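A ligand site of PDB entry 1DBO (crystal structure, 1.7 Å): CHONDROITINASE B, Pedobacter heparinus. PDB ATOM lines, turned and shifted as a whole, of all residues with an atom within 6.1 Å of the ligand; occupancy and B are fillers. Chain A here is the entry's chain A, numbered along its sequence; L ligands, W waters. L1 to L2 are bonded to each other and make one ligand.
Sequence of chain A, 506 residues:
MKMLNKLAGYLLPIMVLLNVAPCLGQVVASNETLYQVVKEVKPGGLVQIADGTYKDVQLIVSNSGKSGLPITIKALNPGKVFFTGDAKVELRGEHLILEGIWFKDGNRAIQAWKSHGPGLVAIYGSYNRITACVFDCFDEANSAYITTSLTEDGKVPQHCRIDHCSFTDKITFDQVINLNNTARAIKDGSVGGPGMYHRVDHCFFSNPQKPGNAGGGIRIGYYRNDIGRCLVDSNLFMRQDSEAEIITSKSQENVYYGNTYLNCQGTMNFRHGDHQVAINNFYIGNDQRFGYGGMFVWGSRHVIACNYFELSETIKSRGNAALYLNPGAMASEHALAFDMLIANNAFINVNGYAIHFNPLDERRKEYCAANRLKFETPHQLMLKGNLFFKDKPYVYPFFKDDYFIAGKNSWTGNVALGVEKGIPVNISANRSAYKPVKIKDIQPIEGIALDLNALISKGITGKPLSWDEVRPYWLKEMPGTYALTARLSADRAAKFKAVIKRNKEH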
ATOM      1  N   GLY A 212      -1.311  25.045 -29.598  1.00  0.00           N
ATOM      2  CA  GLY A 212      -2.631  25.533 -29.955  1.00  0.00           C
ATOM      3  C   GLY A 212      -3.758  24.521 -30.139  1.00  0.00           C
ATOM      4  O   GLY A 212      -3.757  23.455 -29.523  1.00  0.00           O
ATOM      5  N   ASN A 213      -4.718  24.874 -30.985  1.00  0.00           N
ATOM      6  CA  ASN A 213      -5.865  24.013 -31.259  1.00  0.00           C
ATOM      7  C   ASN A 213      -5.435  23.059 -32.383  1.00  0.00           C
ATOM      8  O   ASN A 213      -5.959  23.095 -33.497  1.00  0.00           O
ATOM      9  CB  ASN A 213      -7.066  24.854 -31.716  1.00  0.00           C
ATOM     10  CG  ASN A 213      -7.319  26.049 -30.810  1.00  0.00           C
ATOM     11  OD1 ASN A 213      -6.773  27.141 -31.013  1.00  0.00           O
ATOM     12  ND2 ASN A 213      -8.138  25.835 -29.781  1.00  0.00           N
ATOM     13  N   GLU A 243      -3.810  18.122 -27.364  1.00  0.00           N
ATOM     14  CA  GLU A 243      -4.167  19.521 -27.181  1.00  0.00           C
ATOM     15  C   GLU A 243      -5.137  19.676 -26.026  1.00  0.00           C
ATOM     16  O   GLU A 243      -5.372  18.731 -25.276  1.00  0.00           O
ATOM     17  CB  GLU A 243      -4.787  20.129 -28.453  1.00  0.00           C
ATOM     18  CG  GLU A 243      -6.053  19.457 -28.969  1.00  0.00           C
ATOM     19  CD  GLU A 243      -7.115  20.474 -29.344  1.00  0.00           C
ATOM     20  OE1 GLU A 243      -7.758  21.021 -28.423  1.00  0.00           O
ATOM     21  OE2 GLU A 243      -7.282  20.757 -30.552  1.00  0.00           O
ATOM     22  N   ALA A 244      -5.700  20.876 -25.873  1.00  0.00           N
ATOM     23  CA  ALA A 244      -6.622  21.159 -24.785  1.00  0.00           C
ATOM     24  C   ALA A 244      -7.815  20.195 -24.730  1.00  0.00           C
ATOM     25  O   ALA A 244      -8.316  19.889 -23.650  1.00  0.00           O
ATOM     26  CB  ALA A 244      -7.124  22.588 -24.904  1.00  0.00           C
ATOM     27  N   GLU A 245      -8.248  19.722 -25.888  1.00  0.00           N
ATOM     28  CA  GLU A 245      -9.393  18.822 -25.977  1.00  0.00           C
ATOM     29  C   GLU A 245      -9.035  17.345 -26.150  1.00  0.00           C
ATOM     30  O   GLU A 245      -8.469  16.954 -27.171  1.00  0.00           O
ATOM     31  CB  GLU A 245     -10.310  19.281 -27.112  1.00  0.00           C
ATOM     32  CG  GLU A 245     -10.839  20.694 -26.914  1.00  0.00           C
ATOM     33  CD  GLU A 245     -11.912  21.083 -27.919  1.00  0.00           C
ATOM     34  OE1 GLU A 245     -11.574  21.515 -29.045  1.00  0.00           O
ATOM     35  OE2 GLU A 245     -13.106  20.937 -27.574  1.00  0.00           O
ATOM     36  N   LYS A 250     -18.705  17.420 -30.957  1.00  0.00           N
ATOM     37  CA  LYS A 250     -19.411  18.490 -31.664  1.00  0.00           C
ATOM     38  C   LYS A 250     -20.709  18.051 -32.345  1.00  0.00           C
ATOM     39  O   LYS A 250     -20.971  18.406 -33.494  1.00  0.00           O
ATOM     40  CB  LYS A 250     -18.479  19.117 -32.705  1.00  0.00           C
ATOM     41  CG  LYS A 250     -17.282  19.850 -32.098  1.00  0.00           C
ATOM     42  CD  LYS A 250     -16.412  20.511 -33.155  1.00  0.00           C
ATOM     43  CE  LYS A 250     -15.291  21.316 -32.522  1.00  0.00           C
ATOM     44  NZ  LYS A 250     -14.449  22.011 -33.545  1.00  0.00           N
ATOM     45  N   ASN A 269     -14.671  17.172 -23.667  1.00  0.00           N
ATOM     46  CA  ASN A 269     -15.667  18.221 -23.888  1.00  0.00           C
ATOM     47  C   ASN A 269     -16.954  17.986 -24.665  1.00  0.00           C
ATOM     48  O   ASN A 269     -16.994  17.233 -25.644  1.00  0.00           O
ATOM     49  CB  ASN A 269     -15.010  19.431 -24.584  1.00  0.00           C
ATOM     50  CG  ASN A 269     -13.766  19.919 -23.894  1.00  0.00           C
ATOM     51  OD1 ASN A 269     -13.578  19.719 -22.710  1.00  0.00           O
ATOM     52  ND2 ASN A 269     -12.911  20.603 -24.656  1.00  0.00           N
ATOM     53  N   ARG A 271     -18.415  20.136 -26.670  1.00  0.00           N
ATOM     54  CA  ARG A 271     -18.075  21.387 -27.362  1.00  0.00           C
ATOM     55  C   ARG A 271     -19.225  22.053 -28.116  1.00  0.00           C
ATOM     56  O   ARG A 271     -19.453  23.253 -27.958  1.00  0.00           O
ATOM     57  CB  ARG A 271     -16.906  21.150 -28.318  1.00  0.00           C
ATOM     58  CG  ARG A 271     -16.417  22.409 -29.009  1.00  0.00           C
ATOM     59  CD  ARG A 271     -15.793  23.407 -28.030  1.00  0.00           C
ATOM     60  NE  ARG A 271     -15.509  24.674 -28.692  1.00  0.00           N
ATOM     61  CZ  ARG A 271     -16.420  25.615 -28.941  1.00  0.00           C
ATOM     62  NH1 ARG A 271     -17.679  25.425 -28.571  1.00  0.00           N
ATOM     63  NH2 ARG A 271     -16.078  26.715 -29.592  1.00  0.00           N
ATOM     64  N   HIS A 272     -19.916  21.290 -28.957  1.00  0.00           N
ATOM     65  CA  HIS A 272     -21.068  21.811 -29.703  1.00  0.00           C
ATOM     66  C   HIS A 272     -22.151  20.747 -29.627  1.00  0.00           C
ATOM     67  O   HIS A 272     -21.840  19.556 -29.614  1.00  0.00           O
ATOM     68  CB  HIS A 272     -20.738  22.047 -31.181  1.00  0.00           C
ATOM     69  CG  HIS A 272     -19.786  23.169 -31.432  1.00  0.00           C
ATOM     70  ND1 HIS A 272     -20.041  24.464 -31.040  1.00  0.00           N
ATOM     71  CD2 HIS A 272     -18.613  23.204 -32.109  1.00  0.00           C
ATOM     72  CE1 HIS A 272     -19.058  25.251 -31.462  1.00  0.00           C
ATOM     73  NE2 HIS A 272     -18.186  24.511 -32.115  1.00  0.00           N
ATOM     74  N   PHE A 296     -14.999  20.021 -19.914  1.00  0.00           N
ATOM     75  CA  PHE A 296     -15.378  21.425 -20.125  1.00  0.00           C
ATOM     76  C   PHE A 296     -16.688  21.293 -20.887  1.00  0.00           C
ATOM     77  O   PHE A 296     -16.728  20.655 -21.937  1.00  0.00           O
ATOM     78  CB  PHE A 296     -14.343  22.174 -20.965  1.00  0.00           C
ATOM     79  CG  PHE A 296     -14.344  23.669 -20.752  1.00  0.00           C
ATOM     80  CD1 PHE A 296     -13.297  24.294 -20.078  1.00  0.00           C
ATOM     81  CD2 PHE A 296     -15.393  24.455 -21.232  1.00  0.00           C
ATOM     82  CE1 PHE A 296     -13.283  25.672 -19.897  1.00  0.00           C
ATOM     83  CE2 PHE A 296     -15.386  25.839 -21.052  1.00  0.00           C
ATOM     84  CZ  PHE A 296     -14.324  26.449 -20.385  1.00  0.00           C
ATOM     85  N   TRP A 298     -20.123  22.938 -22.766  1.00  0.00           N
ATOM     86  CA  TRP A 298     -20.828  24.011 -23.463  1.00  0.00           C
ATOM     87  C   TRP A 298     -22.226  23.420 -23.726  1.00  0.00           C
ATOM     88  O   TRP A 298     -22.393  22.207 -23.747  1.00  0.00           O
ATOM     89  CB  TRP A 298     -20.182  24.297 -24.824  1.00  0.00           C
ATOM     90  CG  TRP A 298     -18.872  25.027 -24.833  1.00  0.00           C
ATOM     91  CD1 TRP A 298     -18.679  26.363 -25.084  1.00  0.00           C
ATOM     92  CD2 TRP A 298     -17.567  24.462 -24.683  1.00  0.00           C
ATOM     93  NE1 TRP A 298     -17.333  26.652 -25.112  1.00  0.00           N
ATOM     94  CE2 TRP A 298     -16.626  25.501 -24.881  1.00  0.00           C
ATOM     95  CE3 TRP A 298     -17.095  23.169 -24.423  1.00  0.00           C
ATOM     96  CZ2 TRP A 298     -15.243  25.291 -24.809  1.00  0.00           C
ATOM     97  CZ3 TRP A 298     -15.713  22.956 -24.361  1.00  0.00           C
ATOM     98  CH2 TRP A 298     -14.808  24.016 -24.552  1.00  0.00           C
ATOM     99  N   ARG A 318      -7.242  26.877 -18.032  1.00  0.00           N
ATOM    100  CA  ARG A 318      -8.700  26.837 -18.076  1.00  0.00           C
ATOM    101  C   ARG A 318      -9.406  27.254 -16.786  1.00  0.00           C
ATOM    102  O   ARG A 318     -10.620  27.462 -16.793  1.00  0.00           O
ATOM    103  CB  ARG A 318      -9.152  25.437 -18.530  1.00  0.00           C
ATOM    104  CG  ARG A 318      -8.719  25.084 -19.970  1.00  0.00           C
ATOM    105  CD  ARG A 318      -9.263  26.123 -20.946  1.00  0.00           C
ATOM    106  NE  ARG A 318      -8.967  25.892 -22.370  1.00  0.00           N
ATOM    107  CZ  ARG A 318      -7.785  26.055 -22.957  1.00  0.00           C
ATOM    108  NH1 ARG A 318      -6.732  26.466 -22.257  1.00  0.00           N
ATOM    109  NH2 ARG A 318      -7.662  25.857 -24.267  1.00  0.00           N
ATOM    110  N   ASN A 326     -19.230  26.218 -19.010  1.00  0.00           N
ATOM    111  CA  ASN A 326     -19.071  27.387 -19.858  1.00  0.00           C
ATOM    112  C   ASN A 326     -20.042  28.547 -19.778  1.00  0.00           C
ATOM    113  O   ASN A 326     -21.252  28.360 -19.919  1.00  0.00           O
ATOM    114  CB  ASN A 326     -19.019  26.972 -21.325  1.00  0.00           C
ATOM    115  CG  ASN A 326     -18.665  28.132 -22.231  1.00  0.00           C
ATOM    116  OD1 ASN A 326     -17.531  28.620 -22.198  1.00  0.00           O
ATOM    117  ND2 ASN A 326     -19.622  28.595 -23.023  1.00  0.00           N
ATOM    118  N   GLU A 333     -21.566  29.922 -30.711  1.00  0.00           N
ATOM    119  CA  GLU A 333     -20.325  29.208 -31.047  1.00  0.00           C
ATOM    120  C   GLU A 333     -19.658  28.726 -29.759  1.00  0.00           C
ATOM    121  O   GLU A 333     -18.879  27.776 -29.771  1.00  0.00           O
ATOM    122  CB  GLU A 333     -19.379  30.156 -31.791  1.00  0.00           C
ATOM    123  CG  GLU A 333     -17.943  29.661 -32.018  1.00  0.00           C
ATOM    124  CD  GLU A 333     -17.816  28.666 -33.147  1.00  0.00           C
ATOM    125  OE1 GLU A 333     -18.231  28.997 -34.272  1.00  0.00           O
ATOM    126  OE2 GLU A 333     -17.284  27.553 -32.928  1.00  0.00           O
ATOM    127  N   HIS A 334     -19.941  29.436 -28.671  1.00  0.00           N
ATOM    128  CA  HIS A 334     -19.433  29.105 -27.333  1.00  0.00           C
ATOM    129  C   HIS A 334     -20.688  29.101 -26.474  1.00  0.00           C
ATOM    130  O   HIS A 334     -20.869  29.945 -25.592  1.00  0.00           O
ATOM    131  CB  HIS A 334     -18.435  30.147 -26.840  1.00  0.00           C
ATOM    132  CG  HIS A 334     -17.060  29.990 -27.403  1.00  0.00           C
ATOM    133  ND1 HIS A 334     -16.232  28.931 -27.067  1.00  0.00           N
ATOM    134  CD2 HIS A 334     -16.384  30.708 -28.331  1.00  0.00           C
ATOM    135  CE1 HIS A 334     -15.114  29.007 -27.763  1.00  0.00           C
ATOM    136  NE2 HIS A 334     -15.177  30.077 -28.532  1.00  0.00           N
ATOM    137  N   LEU A 360     -13.109  31.177 -18.047  1.00  0.00           N
ATOM    138  CA  LEU A 360     -12.836  31.987 -19.218  1.00  0.00           C
ATOM    139  C   LEU A 360     -13.899  33.068 -19.434  1.00  0.00           C
ATOM    140  O   LEU A 360     -14.123  33.489 -20.572  1.00  0.00           O
ATOM    141  CB  LEU A 360     -12.762  31.098 -20.456  1.00  0.00           C
ATOM    142  CG  LEU A 360     -11.788  29.921 -20.407  1.00  0.00           C
ATOM    143  CD1 LEU A 360     -11.863  29.140 -21.708  1.00  0.00           C
ATOM    144  CD2 LEU A 360     -10.369  30.423 -20.153  1.00  0.00           C
ATOM    145  N   ARG A 363     -12.808  36.305 -21.458  1.00  0.00           N
ATOM    146  CA  ARG A 363     -12.756  36.151 -22.911  1.00  0.00           C
ATOM    147  C   ARG A 363     -14.154  36.022 -23.514  1.00  0.00           C
ATOM    148  O   ARG A 363     -14.441  36.573 -24.580  1.00  0.00           O
ATOM    149  CB  ARG A 363     -11.978  34.895 -23.308  1.00  0.00           C
ATOM    150  CG  ARG A 363     -10.563  34.792 -22.841  1.00  0.00           C
ATOM    151  CD  ARG A 363     -10.080  33.457 -23.389  1.00  0.00           C
ATOM    152  NE  ARG A 363      -8.807  32.998 -22.851  1.00  0.00           N
ATOM    153  CZ  ARG A 363      -8.333  31.783 -23.079  1.00  0.00           C
ATOM    154  NH1 ARG A 363      -9.039  30.941 -23.825  1.00  0.00           N
ATOM    155  NH2 ARG A 363      -7.175  31.400 -22.566  1.00  0.00           N
ATOM    156  N   ARG A 364     -15.000  35.249 -22.843  1.00  0.00           N
ATOM    157  CA  ARG A 364     -16.366  35.027 -23.309  1.00  0.00           C
ATOM    158  C   ARG A 364     -17.183  36.307 -23.341  1.00  0.00           C
ATOM    159  O   ARG A 364     -17.992  36.513 -24.248  1.00  0.00           O
ATOM    160  CB  ARG A 364     -17.060  34.003 -22.422  1.00  0.00           C
ATOM    161  CG  ARG A 364     -16.482  32.613 -22.494  1.00  0.00           C
ATOM    162  CD  ARG A 364     -16.865  31.872 -23.770  1.00  0.00           C
ATOM    163  NE  ARG A 364     -16.397  30.489 -23.683  1.00  0.00           N
ATOM    164  CZ  ARG A 364     -15.200  30.063 -24.083  1.00  0.00           C
ATOM    165  NH1 ARG A 364     -14.316  30.911 -24.621  1.00  0.00           N
ATOM    166  NH2 ARG A 364     -14.863  28.798 -23.886  1.00  0.00           N
ATOM    167  N   TYR A 367     -16.027  38.173 -26.308  1.00  0.00           N
ATOM    168  CA  TYR A 367     -16.485  37.466 -27.506  1.00  0.00           C
ATOM    169  C   TYR A 367     -17.941  37.844 -27.806  1.00  0.00           C
ATOM    170  O   TYR A 367     -18.297  38.147 -28.947  1.00  0.00           O
ATOM    171  CB  TYR A 367     -16.402  35.951 -27.293  1.00  0.00           C
ATOM    172  CG  TYR A 367     -16.960  35.131 -28.436  1.00  0.00           C
ATOM    173  CD1 TYR A 367     -16.259  35.001 -29.637  1.00  0.00           C
ATOM    174  CD2 TYR A 367     -18.198  34.496 -28.311  1.00  0.00           C
ATOM    175  CE1 TYR A 367     -16.781  34.243 -30.694  1.00  0.00           C
ATOM    176  CE2 TYR A 367     -18.720  33.741 -29.359  1.00  0.00           C
ATOM    177  CZ  TYR A 367     -18.010  33.611 -30.539  1.00  0.00           C
ATOM    178  OH  TYR A 367     -18.530  32.863 -31.558  1.00  0.00           O
HETATM  179  C1  LIG L   1     -12.361  26.298 -30.271  1.00  0.00           C
HETATM  180  C2  LIG L   1     -12.050  27.774 -30.006  1.00  0.00           C
HETATM  181  C3  LIG L   1     -10.776  27.878 -29.163  1.00  0.00           C
HETATM  182  C4  LIG L   1     -10.866  26.992 -27.907  1.00  0.00           C
HETATM  183  C5  LIG L   1     -11.245  25.551 -28.292  1.00  0.00           C
HETATM  184  C6  LIG L   1     -11.473  24.656 -27.100  1.00  0.00           C
HETATM  185  C7  LIG L   1     -12.421  29.685 -31.482  1.00  0.00           C
HETATM  186  C8  LIG L   1     -12.174  30.353 -32.790  1.00  0.00           C
HETATM  187  O1  LIG L   1     -13.547  26.190 -30.962  1.00  0.00           O
HETATM  188  N1  LIG L   1     -11.882  28.482 -31.270  1.00  0.00           N
HETATM  189  O2  LIG L   1     -10.568  29.251 -28.772  1.00  0.00           O
HETATM  190  O3  LIG L   1     -11.845  27.535 -27.010  1.00  0.00           O
HETATM  191  O4  LIG L   1     -12.480  25.563 -29.044  1.00  0.00           O
HETATM  192  O5  LIG L   1     -10.262  24.374 -26.420  1.00  0.00           O
HETATM  193  O6  LIG L   1     -13.109  30.278 -30.622  1.00  0.00           O
HETATM  194  O7  LIG L   1     -11.843  29.523 -25.758  1.00  0.00           O
HETATM  195  O8  LIG L   1     -12.503  27.430 -24.785  1.00  0.00           O
HETATM  196  O9  LIG L   1     -10.273  27.909 -25.258  1.00  0.00           O
HETATM  197  S1  LIG L   1     -11.630  28.108 -25.691  1.00  0.00           S
HETATM  198  C1  LG2 L   2      -9.393  29.887 -29.288  1.00  0.00           C
HETATM  199  C2  LG2 L   2      -9.306  31.422 -29.183  1.00  0.00           C
HETATM  200  C3  LG2 L   2      -9.260  31.867 -27.698  1.00  0.00           C
HETATM  201  C4  LG2 L   2      -8.390  30.925 -26.816  1.00  0.00           C
HETATM  202  C5  LG2 L   2      -7.867  29.606 -27.380  1.00  0.00           C
HETATM  203  O1  LG2 L   2      -8.210  29.313 -28.757  1.00  0.00           O
HETATM  204  C6  LG2 L   2      -7.100  28.635 -26.485  1.00  0.00           C
HETATM  205  O2  LG2 L   2      -6.832  28.970 -25.313  1.00  0.00           O
HETATM  206  O3  LG2 L   2      -6.829  27.508 -26.944  1.00  0.00           O
HETATM  207  O4  LG2 L   2      -8.135  31.892 -29.852  1.00  0.00           O
HETATM  208  O5  LG2 L   2     -10.535  31.639 -27.099  1.00  0.00           O
HETATM  209  O   HOH W   1      -8.318  23.716 -28.006  1.00  0.00           O
HETATM  210  O   HOH W   2     -11.010  23.095 -24.095  1.00  0.00           O
HETATM  211  O   HOH W   3     -10.777  23.968 -32.151  1.00  0.00           O
HETATM  212  O   HOH W   4     -11.656  25.576 -22.944  1.00  0.00           O
HETATM  213  O   HOH W   5     -10.010  26.829 -32.784  1.00  0.00           O
HETATM  214  O   HOH W   6     -13.215  23.072 -31.111  1.00  0.00           O
HETATM  215  O   HOH W   7     -12.722  33.423 -28.050  1.00  0.00           O
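An oxygen (O6) of LIG L1 lies within hydrogen-bond range of a ring nitrogen (NE2) of His 334 (2.9 Å). NH2 of Arg 271 is in hydrogen-bond range of O1 of LIG L1 (2.9 Å). The guanidinium group (NH2) of Arg 318 is in salt-bridge range of an oxygen (O3) of LG2 L2. NH1 of Arg 363 is in salt-bridge range of O2 of LG2 L2 (3.3 Å). OD1 of Asn 213 lies close to O1 of LG2 L2. O8 of LIG L1 is in salt-bridge range of NH2 of Arg 364, 2.9 Å away.
The backbone NH (N) of Glu 245 is in hydrogen-bond range of the side-chain carboxylate (OE1) of Glu 243. The guanidinium group (NH2) of Arg 271 lies within salt-bridge range of the side-chain carboxylate (OE2) of Glu 333, 3.6 Å away. The guanidinium group (NH2) of Arg 271 sits close to a ring nitrogen (ND1) of His 334. The guanidinium group (NE) of Arg 364 sits at hydrogen-bond distance from the side-chain amide oxygen (OD1) of Asn 326, at 2.6 Å. O of His 334 lies within hydrogen-bond range of ND2 of Asn 326 (3.2 Å). The guanidinium group of Arg 364 sits close to a ring nitrogen (ND1) of His 334, at 3.5 Å. ND1 of His 334 lies within hydrogen-bond range of NE1 of Trp 298 (3.2 Å). The side-chain amide nitrogen (ND2) of Asn 269 sits at hydrogen-bond distance from the side-chain carboxylate (OE2) of Glu 245, at 2.9 Å.
Ala 244 touches the ligand. Glu 245 touches the ligand. Trp 298 touches the ligand. CD1 of Leu 360 touches O8 of LIG L1, 3.6 Å away. Ten residues have an atom within 4 Å of the ligand: Asn 213, Ala 244, Glu 245, Arg 271, Trp 298, Arg 318, His 334, Leu 360, Arg 363 and Arg 364. Along chain A the residues within 4 Å of the ligand span positions 213 to 364.
Water W1 lies within hydrogen-bond range of an oxygen (O5) of LIG L1 (2.6 Å), the side-chain amide nitrogen (ND2) of Asn 213 (2.8 Å) and the side-chain carboxylate (OE1) of Glu 243 (2.8 Å). Water W4 lies within hydrogen-bond range of O8 of LIG L1 (2.7 Å) and NE of Arg 318 (2.8 Å). Water W2 bridges an oxygen (O5) of LIG L1 and the side-chain amide nitrogen of Asn 269. Water W6 lies within hydrogen-bond range of NZ of Lys 250 (2.9 Å), OE1 of Glu 245 (3.1 Å) and O1 of LIG L1 (3.1 Å).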
